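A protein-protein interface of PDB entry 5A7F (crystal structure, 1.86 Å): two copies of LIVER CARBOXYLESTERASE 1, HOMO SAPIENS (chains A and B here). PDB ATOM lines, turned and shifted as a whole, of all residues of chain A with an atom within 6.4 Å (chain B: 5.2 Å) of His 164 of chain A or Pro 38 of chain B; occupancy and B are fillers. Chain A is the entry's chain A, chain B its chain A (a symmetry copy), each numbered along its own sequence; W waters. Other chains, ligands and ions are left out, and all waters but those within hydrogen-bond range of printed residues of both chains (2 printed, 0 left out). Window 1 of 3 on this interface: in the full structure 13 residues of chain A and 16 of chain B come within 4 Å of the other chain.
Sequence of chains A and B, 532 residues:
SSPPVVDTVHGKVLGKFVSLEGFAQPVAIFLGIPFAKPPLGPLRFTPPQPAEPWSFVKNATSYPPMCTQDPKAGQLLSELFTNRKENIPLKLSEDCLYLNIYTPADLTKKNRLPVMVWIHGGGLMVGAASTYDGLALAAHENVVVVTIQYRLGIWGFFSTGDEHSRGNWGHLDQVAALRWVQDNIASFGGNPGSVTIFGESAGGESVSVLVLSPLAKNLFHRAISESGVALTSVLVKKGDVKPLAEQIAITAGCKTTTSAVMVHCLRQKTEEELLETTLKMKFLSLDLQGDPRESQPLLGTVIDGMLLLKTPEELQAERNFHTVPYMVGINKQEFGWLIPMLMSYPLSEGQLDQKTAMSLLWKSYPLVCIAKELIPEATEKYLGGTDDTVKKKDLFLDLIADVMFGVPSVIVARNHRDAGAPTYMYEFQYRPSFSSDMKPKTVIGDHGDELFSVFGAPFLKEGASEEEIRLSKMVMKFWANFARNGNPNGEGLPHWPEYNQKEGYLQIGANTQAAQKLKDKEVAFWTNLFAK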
ATOM      1  N   PHE A  45      -8.438   7.669  -3.715  1.00  0.00           N
ATOM      2  CA  PHE A  45      -9.024   8.553  -2.687  1.00  0.00           C
ATOM      3  C   PHE A  45     -10.557   8.491  -2.746  1.00  0.00           C
ATOM      4  O   PHE A  45     -11.219   9.520  -2.666  1.00  0.00           O
ATOM      5  CB  PHE A  45      -8.600   9.989  -2.873  1.00  0.00           C
ATOM      6  CG  PHE A  45      -7.133  10.156  -3.159  1.00  0.00           C
ATOM      7  CD1 PHE A  45      -6.189   9.564  -2.321  1.00  0.00           C
ATOM      8  CD2 PHE A  45      -6.695  10.821  -4.290  1.00  0.00           C
ATOM      9  CE1 PHE A  45      -4.852   9.720  -2.563  1.00  0.00           C
ATOM     10  CE2 PHE A  45      -5.332  10.975  -4.545  1.00  0.00           C
ATOM     11  CZ  PHE A  45      -4.402  10.410  -3.681  1.00  0.00           C
ATOM     12  N   THR A 160      -8.335  15.849   2.909  1.00  0.00           N
ATOM     13  CA  THR A 160      -8.401  17.305   2.848  1.00  0.00           C
ATOM     14  C   THR A 160      -9.213  17.889   4.014  1.00  0.00           C
ATOM     15  O   THR A 160      -9.364  19.097   4.101  1.00  0.00           O
ATOM     16  CB  THR A 160      -9.060  17.787   1.540  1.00  0.00           C
ATOM     17  OG1 THR A 160     -10.333  17.124   1.326  1.00  0.00           O
ATOM     18  CG2 THR A 160      -8.161  17.565   0.373  1.00  0.00           C
ATOM     19  N   ASP A 162     -12.343  17.573   4.309  1.00  0.00           N
ATOM     20  CA  ASP A 162     -13.720  17.864   3.854  1.00  0.00           C
ATOM     21  C   ASP A 162     -14.158  16.811   2.842  1.00  0.00           C
ATOM     22  O   ASP A 162     -13.468  15.788   2.656  1.00  0.00           O
ATOM     23  CB  ASP A 162     -13.780  19.281   3.279  1.00  0.00           C
ATOM     24  CG  ASP A 162     -12.857  19.457   2.066  1.00  0.00           C
ATOM     25  OD1 ASP A 162     -12.640  18.477   1.284  1.00  0.00           O
ATOM     26  OD2 ASP A 162     -12.341  20.587   1.885  1.00  0.00           O
ATOM     27  N   GLU A 163     -15.281  17.087   2.178  1.00  0.00           N
ATOM     28  CA  GLU A 163     -15.992  16.089   1.404  1.00  0.00           C
ATOM     29  C   GLU A 163     -15.279  15.688   0.122  1.00  0.00           C
ATOM     30  O   GLU A 163     -15.617  14.669  -0.468  1.00  0.00           O
ATOM     31  CB  GLU A 163     -17.415  16.552   1.095  1.00  0.00           C
ATOM     32  CG  GLU A 163     -17.518  17.694   0.084  1.00  0.00           C
ATOM     33  CD  GLU A 163     -17.380  19.081   0.705  1.00  0.00           C
ATOM     34  OE1 GLU A 163     -16.894  19.196   1.851  1.00  0.00           O
ATOM     35  OE2 GLU A 163     -17.773  20.054   0.051  1.00  0.00           O
ATOM     36  N   HIS A 164     -14.294  16.478  -0.301  1.00  0.00           N
ATOM     37  CA  HIS A 164     -13.544  16.165  -1.507  1.00  0.00           C
ATOM     38  C   HIS A 164     -12.510  15.063  -1.307  1.00  0.00           C
ATOM     39  O   HIS A 164     -12.130  14.456  -2.300  1.00  0.00           O
ATOM     40  CB  HIS A 164     -12.855  17.388  -2.062  1.00  0.00           C
ATOM     41  CG  HIS A 164     -13.793  18.508  -2.338  1.00  0.00           C
ATOM     42  ND1 HIS A 164     -14.757  18.438  -3.317  1.00  0.00           N
ATOM     43  CD2 HIS A 164     -13.976  19.688  -1.708  1.00  0.00           C
ATOM     44  CE1 HIS A 164     -15.481  19.545  -3.289  1.00  0.00           C
ATOM     45  NE2 HIS A 164     -15.018  20.320  -2.334  1.00  0.00           N
ATOM     46  N   SER A 165     -12.041  14.838  -0.069  1.00  0.00           N
ATOM     47  CA  SER A 165     -11.232  13.655   0.259  1.00  0.00           C
ATOM     48  C   SER A 165     -11.296  13.427   1.752  1.00  0.00           C
ATOM     49  O   SER A 165     -10.473  13.912   2.496  1.00  0.00           O
ATOM     50  CB  SER A 165      -9.781  13.771  -0.250  1.00  0.00           C
ATOM     51  OG  SER A 165      -9.069  12.543  -0.032  1.00  0.00           O
ATOM     52  N   ARG A 166     -12.370  12.767   2.185  1.00  0.00           N
ATOM     53  CA  ARG A 166     -12.642  12.626   3.593  1.00  0.00           C
ATOM     54  C   ARG A 166     -11.495  11.972   4.321  1.00  0.00           C
ATOM     55  O   ARG A 166     -11.145  12.400   5.414  1.00  0.00           O
ATOM     56  CB  ARG A 166     -13.908  11.792   3.836  1.00  0.00           C
ATOM     57  CG  ARG A 166     -15.196  12.557   3.621  1.00  0.00           C
ATOM     58  CD  ARG A 166     -16.353  11.695   4.085  1.00  0.00           C
ATOM     59  NE  ARG A 166     -17.576  12.455   4.258  1.00  0.00           N
ATOM     60  CZ  ARG A 166     -18.384  12.829   3.285  1.00  0.00           C
ATOM     61  NH1 ARG A 166     -18.105  12.513   2.023  1.00  0.00           N
ATOM     62  NH2 ARG A 166     -19.480  13.541   3.583  1.00  0.00           N
ATOM     63  N   TRP A 169      -9.405   5.846   3.676  1.00  0.00           N
ATOM     64  CA  TRP A 169      -9.670   4.919   2.570  1.00  0.00           C
ATOM     65  C   TRP A 169      -9.199   3.526   3.007  1.00  0.00           C
ATOM     66  O   TRP A 169      -9.867   2.566   2.725  1.00  0.00           O
ATOM     67  CB  TRP A 169      -8.884   5.397   1.314  1.00  0.00           C
ATOM     68  CG  TRP A 169      -9.075   6.866   1.082  1.00  0.00           C
ATOM     69  CD1 TRP A 169      -8.086   7.873   1.062  1.00  0.00           C
ATOM     70  CD2 TRP A 169     -10.327   7.530   0.875  1.00  0.00           C
ATOM     71  NE1 TRP A 169      -8.690   9.080   0.835  1.00  0.00           N
ATOM     72  CE2 TRP A 169     -10.060   8.900   0.747  1.00  0.00           C
ATOM     73  CE3 TRP A 169     -11.670   7.084   0.813  1.00  0.00           C
ATOM     74  CZ2 TRP A 169     -11.083   9.844   0.532  1.00  0.00           C
ATOM     75  CZ3 TRP A 169     -12.678   8.007   0.614  1.00  0.00           C
ATOM     76  CH2 TRP A 169     -12.377   9.377   0.454  1.00  0.00           C
ATOM     77  N   THR A 258      -7.668  24.940  -3.873  1.00  0.00           N
ATOM     78  CA  THR A 258      -8.829  24.384  -3.160  1.00  0.00           C
ATOM     79  C   THR A 258      -8.584  22.894  -2.897  1.00  0.00           C
ATOM     80  O   THR A 258      -7.659  22.278  -3.457  1.00  0.00           O
ATOM     81  CB  THR A 258     -10.129  24.461  -3.952  1.00  0.00           C
ATOM     82  OG1 THR A 258     -10.132  23.489  -5.007  1.00  0.00           O
ATOM     83  CG2 THR A 258     -10.383  25.843  -4.499  1.00  0.00           C
ATOM     84  N   SER A 259      -9.392  22.347  -2.012  1.00  0.00           N
ATOM     85  CA  SER A 259      -9.377  20.938  -1.737  1.00  0.00           C
ATOM     86  C   SER A 259      -9.561  20.100  -2.994  1.00  0.00           C
ATOM     87  O   SER A 259      -8.803  19.152  -3.217  1.00  0.00           O
ATOM     88  CB  SER A 259     -10.485  20.571  -0.733  1.00  0.00           C
ATOM     89  OG  SER A 259     -10.222  21.082   0.561  1.00  0.00           O
ATOM     90  N   ALA A 260     -10.590  20.428  -3.775  1.00  0.00           N
ATOM     91  CA  ALA A 260     -10.939  19.637  -4.966  1.00  0.00           C
ATOM     92  C   ALA A 260      -9.801  19.709  -5.989  1.00  0.00           C
ATOM     93  O   ALA A 260      -9.491  18.721  -6.662  1.00  0.00           O
ATOM     94  CB  ALA A 260     -12.257  20.111  -5.574  1.00  0.00           C
ATOM     95  N   VAL A 261      -9.145  20.864  -6.064  1.00  0.00           N
ATOM     96  CA  VAL A 261      -7.972  20.996  -6.940  1.00  0.00           C
ATOM     97  C   VAL A 261      -6.815  20.060  -6.535  1.00  0.00           C
ATOM     98  O   VAL A 261      -6.185  19.431  -7.383  1.00  0.00           O
ATOM     99  CB  VAL A 261      -7.491  22.464  -7.040  1.00  0.00           C
ATOM    100  CG1 VAL A 261      -6.041  22.574  -7.482  1.00  0.00           C
ATOM    101  CG2 VAL A 261      -8.398  23.224  -7.985  1.00  0.00           C
ATOM    102  N   VAL A 263      -6.948  17.249  -4.672  1.00  0.00           N
ATOM    103  CA  VAL A 263      -7.282  15.854  -4.830  1.00  0.00           C
ATOM    104  C   VAL A 263      -7.297  15.465  -6.302  1.00  0.00           C
ATOM    105  O   VAL A 263      -6.838  14.385  -6.647  1.00  0.00           O
ATOM    106  CB  VAL A 263      -8.676  15.472  -4.317  1.00  0.00           C
ATOM    107  CG1 VAL A 263      -8.798  13.961  -4.425  1.00  0.00           C
ATOM    108  CG2 VAL A 263      -8.850  15.899  -2.884  1.00  0.00           C
ATOM    109  N   ARG A 267      -4.856  12.732  -8.138  1.00  0.00           N
ATOM    110  CA  ARG A 267      -5.375  11.638  -8.957  1.00  0.00           C
ATOM    111  C   ARG A 267      -4.747  11.553 -10.338  1.00  0.00           C
ATOM    112  O   ARG A 267      -4.883  10.521 -10.948  1.00  0.00           O
ATOM    113  CB  ARG A 267      -6.875  11.721  -9.192  1.00  0.00           C
ATOM    114  CG  ARG A 267      -7.639  11.360  -7.991  1.00  0.00           C
ATOM    115  CD  ARG A 267      -9.085  11.240  -8.360  1.00  0.00           C
ATOM    116  NE  ARG A 267      -9.815  10.909  -7.146  1.00  0.00           N
ATOM    117  CZ  ARG A 267     -10.759  11.629  -6.572  1.00  0.00           C
ATOM    118  NH1 ARG A 267     -11.198  12.758  -7.107  1.00  0.00           N
ATOM    119  NH2 ARG A 267     -11.280  11.188  -5.459  1.00  0.00           N
ATOM    120  N   ALA B  36     -22.688  23.037  -6.824  1.00  0.00           N
ATOM    121  CA  ALA B  36     -22.490  21.918  -7.732  1.00  0.00           C
ATOM    122  C   ALA B  36     -21.143  21.281  -7.424  1.00  0.00           C
ATOM    123  O   ALA B  36     -20.350  21.830  -6.681  1.00  0.00           O
ATOM    124  CB  ALA B  36     -22.535  22.400  -9.165  1.00  0.00           C
ATOM    125  N   LYS B  37     -20.883  20.150  -8.041  1.00  0.00           N
ATOM    126  CA  LYS B  37     -19.614  19.455  -7.917  1.00  0.00           C
ATOM    127  C   LYS B  37     -18.588  20.205  -8.733  1.00  0.00           C
ATOM    128  O   LYS B  37     -18.886  20.655  -9.841  1.00  0.00           O
ATOM    129  CB  LYS B  37     -19.756  18.038  -8.482  1.00  0.00           C
ATOM    130  CG  LYS B  37     -18.554  17.131  -8.280  1.00  0.00           C
ATOM    131  CD  LYS B  37     -18.969  15.659  -8.379  1.00  0.00           C
ATOM    132  CE  LYS B  37     -17.730  14.771  -8.454  1.00  0.00           C
ATOM    133  NZ  LYS B  37     -18.060  13.308  -8.549  1.00  0.00           N
ATOM    134  N   PRO B  38     -17.371  20.331  -8.224  1.00  0.00           N
ATOM    135  CA  PRO B  38     -16.422  21.056  -9.061  1.00  0.00           C
ATOM    136  C   PRO B  38     -16.304  20.404 -10.441  1.00  0.00           C
ATOM    137  O   PRO B  38     -16.048  19.192 -10.537  1.00  0.00           O
ATOM    138  CB  PRO B  38     -15.105  20.944  -8.274  1.00  0.00           C
ATOM    139  CG  PRO B  38     -15.545  20.842  -6.872  1.00  0.00           C
ATOM    140  CD  PRO B  38     -16.799  20.008  -6.910  1.00  0.00           C
ATOM    141  N   PRO B  39     -16.413  21.209 -11.524  1.00  0.00           N
ATOM    142  CA  PRO B  39     -16.458  20.645 -12.880  1.00  0.00           C
ATOM    143  C   PRO B  39     -15.035  20.312 -13.411  1.00  0.00           C
ATOM    144  O   PRO B  39     -14.596  20.837 -14.445  1.00  0.00           O
ATOM    145  CB  PRO B  39     -17.169  21.778 -13.667  1.00  0.00           C
ATOM    146  CG  PRO B  39     -16.581  23.047 -13.035  1.00  0.00           C
ATOM    147  CD  PRO B  39     -16.421  22.700 -11.554  1.00  0.00           C
ATOM    148  N   LEU B  40     -14.326  19.407 -12.729  1.00  0.00           N
ATOM    149  CA  LEU B  40     -12.933  19.077 -13.075  1.00  0.00           C
ATOM    150  C   LEU B  40     -12.848  17.784 -13.911  1.00  0.00           C
ATOM    151  O   LEU B  40     -13.706  16.920 -13.831  1.00  0.00           O
ATOM    152  CB  LEU B  40     -12.118  18.871 -11.792  1.00  0.00           C
ATOM    153  CG  LEU B  40     -12.251  20.001 -10.778  1.00  0.00           C
ATOM    154  CD1 LEU B  40     -11.422  19.730  -9.532  1.00  0.00           C
ATOM    155  CD2 LEU B  40     -11.891  21.344 -11.383  1.00  0.00           C
ATOM    156  N   LEU B  43     -15.662  16.092 -15.964  1.00  0.00           N
ATOM    157  CA  LEU B  43     -16.783  17.023 -15.841  1.00  0.00           C
ATOM    158  C   LEU B  43     -16.641  18.358 -16.565  1.00  0.00           C
ATOM    159  O   LEU B  43     -17.575  19.167 -16.579  1.00  0.00           O
ATOM    160  CB  LEU B  43     -17.110  17.269 -14.375  1.00  0.00           C
ATOM    161  CG  LEU B  43     -17.519  16.002 -13.613  1.00  0.00           C
ATOM    162  CD1 LEU B  43     -17.804  16.368 -12.170  1.00  0.00           C
ATOM    163  CD2 LEU B  43     -18.742  15.330 -14.247  1.00  0.00           C
ATOM    164  N   ASP B  95     -12.281  25.161 -10.258  1.00  0.00           N
ATOM    165  CA  ASP B  95     -13.177  24.911  -9.113  1.00  0.00           C
ATOM    166  C   ASP B  95     -13.752  26.255  -8.677  1.00  0.00           C
ATOM    167  O   ASP B  95     -13.195  26.915  -7.793  1.00  0.00           O
ATOM    168  CB  ASP B  95     -12.416  24.232  -7.962  1.00  0.00           C
ATOM    169  CG  ASP B  95     -13.271  23.941  -6.749  1.00  0.00           C
ATOM    170  OD1 ASP B  95     -14.516  24.083  -6.784  1.00  0.00           O
ATOM    171  OD2 ASP B  95     -12.671  23.555  -5.735  1.00  0.00           O
ATOM    172  N   TYR B  98     -19.426  28.350  -7.018  1.00  0.00           N
ATOM    173  CA  TYR B  98     -19.804  28.840  -5.712  1.00  0.00           C
ATOM    174  C   TYR B  98     -20.738  30.047  -5.832  1.00  0.00           C
ATOM    175  O   TYR B  98     -20.768  30.754  -6.876  1.00  0.00           O
ATOM    176  CB  TYR B  98     -18.556  29.252  -4.929  1.00  0.00           C
ATOM    177  CG  TYR B  98     -17.640  28.114  -4.696  1.00  0.00           C
ATOM    178  CD1 TYR B  98     -17.856  27.238  -3.638  1.00  0.00           C
ATOM    179  CD2 TYR B  98     -16.678  27.801  -5.611  1.00  0.00           C
ATOM    180  CE1 TYR B  98     -17.051  26.118  -3.458  1.00  0.00           C
ATOM    181  CE2 TYR B  98     -15.878  26.696  -5.461  1.00  0.00           C
ATOM    182  CZ  TYR B  98     -16.046  25.859  -4.384  1.00  0.00           C
ATOM    183  OH  TYR B  98     -15.281  24.715  -4.253  1.00  0.00           O
HETATM  184  O   HOH W   1     -16.762  22.605  -3.382  1.00  0.00           O
HETATM  185  O   HOH W   2     -12.801  22.416  -3.147  1.00  0.00           O
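The side-chain carboxylate (OD2) of Asp 95 of chain B sits at hydrogen-bond distance from the side-chain hydroxyl (OG1) of Thr 258 of chain A.
The side-chain hydroxyl (OG1) of Thr 258 of chain A is in hydrogen-bond range of the backbone NH (N) of Val 261 of chain A (3.0 Å).
OG1 of Thr 258 of chain A sits close to N of Ala 260 of chain A (3.3 Å).
OD1 of Asp 95 of chain B sits at hydrogen-bond distance from OH of Tyr 98 of chain B.
The side-chain carboxylate of Asp 162 of chain A lies within hydrogen-bond range of the backbone NH of His 164 of chain A.
Among the printed residues, pairs that only touch across the chains: His 164 of chain A with Pro 38 of chain B (3.8 Å), Ala 260 of chain A with Pro 38 of chain B (3.6 Å), Ala 260 of chain A with Leu 40 of chain B (3.6 Å) and Ala 260 of chain A with Asp 95 of chain B (3.5 Å).
Of the printed residues of chain B, Ala 260 of chain A touches Pro 38, Leu 40 and Asp 95.
Val 261 of chain A touches none of the printed residues of chain B.
Lys 37 of chain B touches none of the printed residues of chain A.
Of chain A, only His 164 and Ala 260 come within 4 Å of Pro 38 of chain B.
Printed residues of chain A within 4 Å of Leu 40 of chain B: Ala 260 (3.6 Å).
Of the printed residues of chain A, Asp 95 of chain B touches Thr 258 (2.6 Å) and Ala 260 (3.5 Å).
The nearest residue of chain B that does not touch His 164 of chain A is Tyr 98 of chain B (4.8 Å).
Of the 8 printed residues of chain B, 3 touch a printed residue of chain A.
Among the printed residues, 5 pairs touch across the chains.
No position is printed for both chains.
Of the 5 pairs that touch across the chains among the printed residues, none has its exchanged pair printed and touching as well.
Water W1 lies within hydrogen-bond range of the side-chain hydroxyl (OH) of Tyr 98 of chain B (2.7 Å) and a ring nitrogen (NE2) of His 164 of chain A (3.1 Å).
Water W2 lies within hydrogen-bond range of the side-chain carboxylate (OD2) of Asp 95 of chain B, the backbone NH (N) of Ala 260 of chain A, a ring nitrogen (NE2) of His 164 of chain A and the side-chain hydroxyl (OG1) of Thr 258 of chain A.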
